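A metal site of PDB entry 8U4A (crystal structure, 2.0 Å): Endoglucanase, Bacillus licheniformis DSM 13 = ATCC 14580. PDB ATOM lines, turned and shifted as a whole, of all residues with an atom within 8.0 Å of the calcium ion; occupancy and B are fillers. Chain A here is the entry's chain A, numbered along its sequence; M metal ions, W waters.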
ATOM      1  N   THR A 480       6.189   4.955  35.634  1.00  0.00           N
ATOM      2  CA  THR A 480       7.150   5.241  34.579  1.00  0.00           C
ATOM      3  C   THR A 480       7.418   6.723  34.679  1.00  0.00           C
ATOM      4  O   THR A 480       6.468   7.496  34.858  1.00  0.00           O
ATOM      5  CB  THR A 480       6.623   4.932  33.163  1.00  0.00           C
ATOM      6  OG1 THR A 480       6.469   3.533  32.995  1.00  0.00           O
ATOM      7  CG2 THR A 480       7.621   5.470  32.067  1.00  0.00           C
ATOM      8  N   TYR A 505       0.980   8.831  25.495  1.00  0.00           N
ATOM      9  CA  TYR A 505      -0.104   7.862  25.514  1.00  0.00           C
ATOM     10  C   TYR A 505       0.277   6.556  26.178  1.00  0.00           C
ATOM     11  O   TYR A 505       1.391   6.049  25.987  1.00  0.00           O
ATOM     12  CB  TYR A 505      -0.570   7.515  24.104  1.00  0.00           C
ATOM     13  CG  TYR A 505      -1.204   8.667  23.348  1.00  0.00           C
ATOM     14  CD1 TYR A 505      -0.410   9.660  22.725  1.00  0.00           C
ATOM     15  CD2 TYR A 505      -2.588   8.758  23.233  1.00  0.00           C
ATOM     16  CE1 TYR A 505      -1.025  10.712  21.980  1.00  0.00           C
ATOM     17  CE2 TYR A 505      -3.188   9.799  22.519  1.00  0.00           C
ATOM     18  CZ  TYR A 505      -2.419  10.759  21.889  1.00  0.00           C
ATOM     19  OH  TYR A 505      -3.051  11.777  21.189  1.00  0.00           O
ATOM     20  N   VAL A 506      -0.687   5.988  26.904  1.00  0.00           N
ATOM     21  CA  VAL A 506      -0.545   4.740  27.621  1.00  0.00           C
ATOM     22  C   VAL A 506      -1.774   3.876  27.362  1.00  0.00           C
ATOM     23  O   VAL A 506      -2.854   4.350  26.949  1.00  0.00           O
ATOM     24  CB  VAL A 506      -0.333   4.942  29.150  1.00  0.00           C
ATOM     25  CG1 VAL A 506       0.945   5.739  29.414  1.00  0.00           C
ATOM     26  CG2 VAL A 506      -1.553   5.638  29.806  1.00  0.00           C
ATOM     27  N   ASP A 507      -1.564   2.578  27.557  1.00  0.00           N
ATOM     28  CA  ASP A 507      -2.587   1.559  27.500  1.00  0.00           C
ATOM     29  C   ASP A 507      -2.785   1.110  28.943  1.00  0.00           C
ATOM     30  O   ASP A 507      -1.856   0.604  29.569  1.00  0.00           O
ATOM     31  CB  ASP A 507      -2.134   0.398  26.606  1.00  0.00           C
ATOM     32  CG  ASP A 507      -3.211  -0.659  26.381  1.00  0.00           C
ATOM     33  OD1 ASP A 507      -4.151  -0.816  27.207  1.00  0.00           O
ATOM     34  OD2 ASP A 507      -3.091  -1.377  25.359  1.00  0.00           O
ATOM     35  N   LEU A 508      -4.001   1.293  29.463  1.00  0.00           N
ATOM     36  CA  LEU A 508      -4.311   0.893  30.826  1.00  0.00           C
ATOM     37  C   LEU A 508      -5.027  -0.469  30.899  1.00  0.00           C
ATOM     38  O   LEU A 508      -5.645  -0.779  31.910  1.00  0.00           O
ATOM     39  CB  LEU A 508      -5.150   1.966  31.506  1.00  0.00           C
ATOM     40  CG  LEU A 508      -4.445   3.320  31.628  1.00  0.00           C
ATOM     41  CD1 LEU A 508      -5.301   4.324  32.415  1.00  0.00           C
ATOM     42  CD2 LEU A 508      -3.092   3.137  32.315  1.00  0.00           C
ATOM     43  N   THR A 509      -4.891  -1.304  29.860  1.00  0.00           N
ATOM     44  CA  THR A 509      -5.595  -2.585  29.857  1.00  0.00           C
ATOM     45  C   THR A 509      -5.256  -3.416  31.099  1.00  0.00           C
ATOM     46  O   THR A 509      -6.144  -3.951  31.755  1.00  0.00           O
ATOM     47  CB  THR A 509      -5.288  -3.371  28.585  1.00  0.00           C
ATOM     48  OG1 THR A 509      -5.818  -2.669  27.464  1.00  0.00           O
ATOM     49  CG2 THR A 509      -5.953  -4.783  28.616  1.00  0.00           C
ATOM     50  N   GLU A 510      -3.959  -3.549  31.405  1.00  0.00           N
ATOM     51  CA  GLU A 510      -3.499  -4.283  32.583  1.00  0.00           C
ATOM     52  C   GLU A 510      -4.010  -3.688  33.899  1.00  0.00           C
ATOM     53  O   GLU A 510      -4.224  -4.424  34.869  1.00  0.00           O
ATOM     54  CB  GLU A 510      -1.964  -4.350  32.571  1.00  0.00           C
ATOM     55  CG  GLU A 510      -1.235  -3.096  33.052  1.00  0.00           C
ATOM     56  CD  GLU A 510      -0.897  -2.076  31.938  1.00  0.00           C
ATOM     57  OE1 GLU A 510      -1.285  -2.259  30.743  1.00  0.00           O
ATOM     58  OE2 GLU A 510      -0.215  -1.082  32.285  1.00  0.00           O
ATOM     59  N   ALA A 511      -4.191  -2.361  33.955  1.00  0.00           N
ATOM     60  CA  ALA A 511      -4.824  -1.712  35.106  1.00  0.00           C
ATOM     61  C   ALA A 511      -6.270  -2.174  35.285  1.00  0.00           C
ATOM     62  O   ALA A 511      -6.691  -2.619  36.367  1.00  0.00           O
ATOM     63  CB  ALA A 511      -4.773  -0.194  34.899  1.00  0.00           C
ATOM     64  N   HIS A 544      -8.957   1.264  26.421  1.00  0.00           N
ATOM     65  CA  HIS A 544      -8.213   1.707  27.603  1.00  0.00           C
ATOM     66  C   HIS A 544      -6.963   2.511  27.258  1.00  0.00           C
ATOM     67  O   HIS A 544      -5.941   2.440  27.952  1.00  0.00           O
ATOM     68  CB  HIS A 544      -7.861   0.485  28.475  1.00  0.00           C
ATOM     69  CG  HIS A 544      -9.034  -0.412  28.709  1.00  0.00           C
ATOM     70  ND1 HIS A 544     -10.175   0.030  29.347  1.00  0.00           N
ATOM     71  CD2 HIS A 544      -9.265  -1.699  28.339  1.00  0.00           C
ATOM     72  CE1 HIS A 544     -11.055  -0.957  29.385  1.00  0.00           C
ATOM     73  NE2 HIS A 544     -10.543  -2.009  28.756  1.00  0.00           N
ATOM     74  N   ILE A 545      -7.041   3.304  26.185  1.00  0.00           N
ATOM     75  CA  ILE A 545      -5.937   4.153  25.757  1.00  0.00           C
ATOM     76  C   ILE A 545      -6.183   5.566  26.283  1.00  0.00           C
ATOM     77  O   ILE A 545      -7.220   6.167  26.008  1.00  0.00           O
ATOM     78  CB  ILE A 545      -5.771   4.135  24.229  1.00  0.00           C
ATOM     79  CG1 ILE A 545      -5.724   2.678  23.761  1.00  0.00           C
ATOM     80  CG2 ILE A 545      -4.511   4.918  23.791  1.00  0.00           C
ATOM     81  CD1 ILE A 545      -4.572   1.859  24.298  1.00  0.00           C
ATOM     82  N   PHE A 581       0.607  -3.884  38.881  1.00  0.00           N
ATOM     83  CA  PHE A 581       0.120  -4.176  37.536  1.00  0.00           C
ATOM     84  C   PHE A 581       0.764  -3.316  36.453  1.00  0.00           C
ATOM     85  O   PHE A 581       0.758  -3.723  35.308  1.00  0.00           O
ATOM     86  CB  PHE A 581      -1.390  -3.971  37.443  1.00  0.00           C
ATOM     87  CG  PHE A 581      -1.840  -2.617  37.863  1.00  0.00           C
ATOM     88  CD1 PHE A 581      -1.705  -1.526  36.992  1.00  0.00           C
ATOM     89  CD2 PHE A 581      -2.404  -2.417  39.113  1.00  0.00           C
ATOM     90  CE1 PHE A 581      -2.106  -0.245  37.377  1.00  0.00           C
ATOM     91  CE2 PHE A 581      -2.811  -1.137  39.510  1.00  0.00           C
ATOM     92  CZ  PHE A 581      -2.673  -0.055  38.640  1.00  0.00           C
ATOM     93  N   TRP A 582       1.293  -2.137  36.789  1.00  0.00           N
ATOM     94  CA  TRP A 582       1.653  -1.161  35.756  1.00  0.00           C
ATOM     95  C   TRP A 582       2.633  -1.751  34.739  1.00  0.00           C
ATOM     96  O   TRP A 582       3.648  -2.359  35.105  1.00  0.00           O
ATOM     97  CB  TRP A 582       2.231   0.068  36.427  1.00  0.00           C
ATOM     98  CG  TRP A 582       2.760   1.119  35.483  1.00  0.00           C
ATOM     99  CD1 TRP A 582       4.033   1.274  35.075  1.00  0.00           C
ATOM    100  CD2 TRP A 582       2.004   2.151  34.861  1.00  0.00           C
ATOM    101  NE1 TRP A 582       4.142   2.350  34.245  1.00  0.00           N
ATOM    102  CE2 TRP A 582       2.913   2.920  34.098  1.00  0.00           C
ATOM    103  CE3 TRP A 582       0.653   2.533  34.908  1.00  0.00           C
ATOM    104  CZ2 TRP A 582       2.519   4.052  33.333  1.00  0.00           C
ATOM    105  CZ3 TRP A 582       0.252   3.672  34.131  1.00  0.00           C
ATOM    106  CH2 TRP A 582       1.190   4.400  33.372  1.00  0.00           C
ATOM    107  N   ASN A 583       2.302  -1.625  33.462  1.00  0.00           N
ATOM    108  CA  ASN A 583       3.083  -2.223  32.378  1.00  0.00           C
ATOM    109  C   ASN A 583       3.312  -1.244  31.227  1.00  0.00           C
ATOM    110  O   ASN A 583       2.436  -1.059  30.362  1.00  0.00           O
ATOM    111  CB  ASN A 583       2.425  -3.504  31.876  1.00  0.00           C
ATOM    112  CG  ASN A 583       3.177  -4.127  30.710  1.00  0.00           C
ATOM    113  OD1 ASN A 583       4.344  -3.804  30.476  1.00  0.00           O
ATOM    114  ND2 ASN A 583       2.515  -5.025  29.996  1.00  0.00           N
ATOM    115  N   PRO A 584       4.492  -0.639  31.150  1.00  0.00           N
ATOM    116  CA  PRO A 584       4.738   0.338  30.080  1.00  0.00           C
ATOM    117  C   PRO A 584       4.906  -0.281  28.714  1.00  0.00           C
ATOM    118  O   PRO A 584       4.875   0.457  27.719  1.00  0.00           O
ATOM    119  CB  PRO A 584       6.056   1.003  30.517  1.00  0.00           C
ATOM    120  CG  PRO A 584       6.756  -0.107  31.214  1.00  0.00           C
ATOM    121  CD  PRO A 584       5.682  -0.847  31.988  1.00  0.00           C
ATOM    122  N   GLU A 585       5.101  -1.583  28.628  1.00  0.00           N
ATOM    123  CA  GLU A 585       5.537  -2.190  27.375  1.00  0.00           C
ATOM    124  C   GLU A 585       4.455  -2.134  26.317  1.00  0.00           C
ATOM    125  O   GLU A 585       4.784  -2.160  25.133  1.00  0.00           O
ATOM    126  CB  GLU A 585       5.951  -3.649  27.594  1.00  0.00           C
ATOM    127  CG  GLU A 585       7.128  -3.874  28.577  1.00  0.00           C
ATOM    128  CD  GLU A 585       8.412  -3.193  28.128  1.00  0.00           C
ATOM    129  OE1 GLU A 585       8.667  -3.094  26.897  1.00  0.00           O
ATOM    130  OE2 GLU A 585       9.166  -2.754  29.032  1.00  0.00           O
ATOM    131  N   ASN A 586       3.179  -2.050  26.718  1.00  0.00           N
ATOM    132  CA  ASN A 586       2.092  -1.892  25.762  1.00  0.00           C
ATOM    133  C   ASN A 586       1.644  -0.418  25.590  1.00  0.00           C
ATOM    134  O   ASN A 586       0.633  -0.159  24.941  1.00  0.00           O
ATOM    135  CB  ASN A 586       0.924  -2.792  26.176  1.00  0.00           C
ATOM    136  CG  ASN A 586       0.279  -2.375  27.495  1.00  0.00           C
ATOM    137  OD1 ASN A 586       0.684  -1.389  28.143  1.00  0.00           O
ATOM    138  ND2 ASN A 586      -0.737  -3.132  27.921  1.00  0.00           N
ATOM    139  N   ASP A 587       2.418   0.555  26.121  1.00  0.00           N
ATOM    140  CA  ASP A 587       2.081   1.970  26.044  1.00  0.00           C
ATOM    141  C   ASP A 587       2.643   2.579  24.769  1.00  0.00           C
ATOM    142  O   ASP A 587       3.863   2.530  24.542  1.00  0.00           O
ATOM    143  CB  ASP A 587       2.609   2.762  27.241  1.00  0.00           C
ATOM    144  CG  ASP A 587       2.007   2.338  28.542  1.00  0.00           C
ATOM    145  OD1 ASP A 587       0.972   1.649  28.520  1.00  0.00           O
ATOM    146  OD2 ASP A 587       2.558   2.700  29.589  1.00  0.00           O
ATOM    147  N   HIS A 588       1.748   3.173  23.974  1.00  0.00           N
ATOM    148  CA  HIS A 588       2.115   3.750  22.680  1.00  0.00           C
ATOM    149  C   HIS A 588       3.350   4.636  22.784  1.00  0.00           C
ATOM    150  O   HIS A 588       4.298   4.486  22.002  1.00  0.00           O
ATOM    151  CB  HIS A 588       0.908   4.521  22.127  1.00  0.00           C
ATOM    152  CG  HIS A 588       1.152   5.256  20.844  1.00  0.00           C
ATOM    153  ND1 HIS A 588       0.991   4.669  19.602  1.00  0.00           N
ATOM    154  CD2 HIS A 588       1.517   6.542  20.610  1.00  0.00           C
ATOM    155  CE1 HIS A 588       1.256   5.564  18.665  1.00  0.00           C
ATOM    156  NE2 HIS A 588       1.556   6.716  19.253  1.00  0.00           N
ATOM    157  N   TYR A 590       5.763   4.856  25.010  1.00  0.00           N
ATOM    158  CA  TYR A 590       6.956   4.211  25.566  1.00  0.00           C
ATOM    159  C   TYR A 590       7.810   3.507  24.513  1.00  0.00           C
ATOM    160  O   TYR A 590       8.998   3.244  24.783  1.00  0.00           O
ATOM    161  CB  TYR A 590       6.504   3.171  26.585  1.00  0.00           C
ATOM    162  CG  TYR A 590       7.546   2.700  27.557  1.00  0.00           C
ATOM    163  CD1 TYR A 590       8.025   3.542  28.563  1.00  0.00           C
ATOM    164  CD2 TYR A 590       7.992   1.382  27.531  1.00  0.00           C
ATOM    165  CE1 TYR A 590       8.941   3.096  29.484  1.00  0.00           C
ATOM    166  CE2 TYR A 590       8.935   0.928  28.458  1.00  0.00           C
ATOM    167  CZ  TYR A 590       9.394   1.801  29.440  1.00  0.00           C
ATOM    168  OH  TYR A 590      10.308   1.381  30.387  1.00  0.00           O
HETATM  169 CA    CA M   1       0.263  -0.142  30.099  1.00  0.00          CA
HETATM  170  O   HOH W   1       0.838   1.638  31.447  1.00  0.00           O
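The side-chain carboxylate (OD1) of Asp 507 sits at hydrogen-bond distance from the side-chain hydroxyl (OG1) of Thr 509. The backbone NH (N) of Glu 585 sits at hydrogen-bond distance from the side-chain amide oxygen (OD1) of Asn 583 (3.0 Å).
Water W1 binds the calcium ion, at 2.3 Å. O of Asp 507 binds the calcium ion (2.3 Å). OD1 of Asn 586 is bound to the calcium ion, at 2.4 Å. The backbone carbonyl oxygen (O) of Asn 583 binds the calcium ion. The calcium ion is bound by OE2 of Glu 510, 2.4 Å away. OD1 of Asp 587 is bound to the calcium ion, at 2.5 Å. OE1 of Glu 510 binds the calcium ion (2.7 Å).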
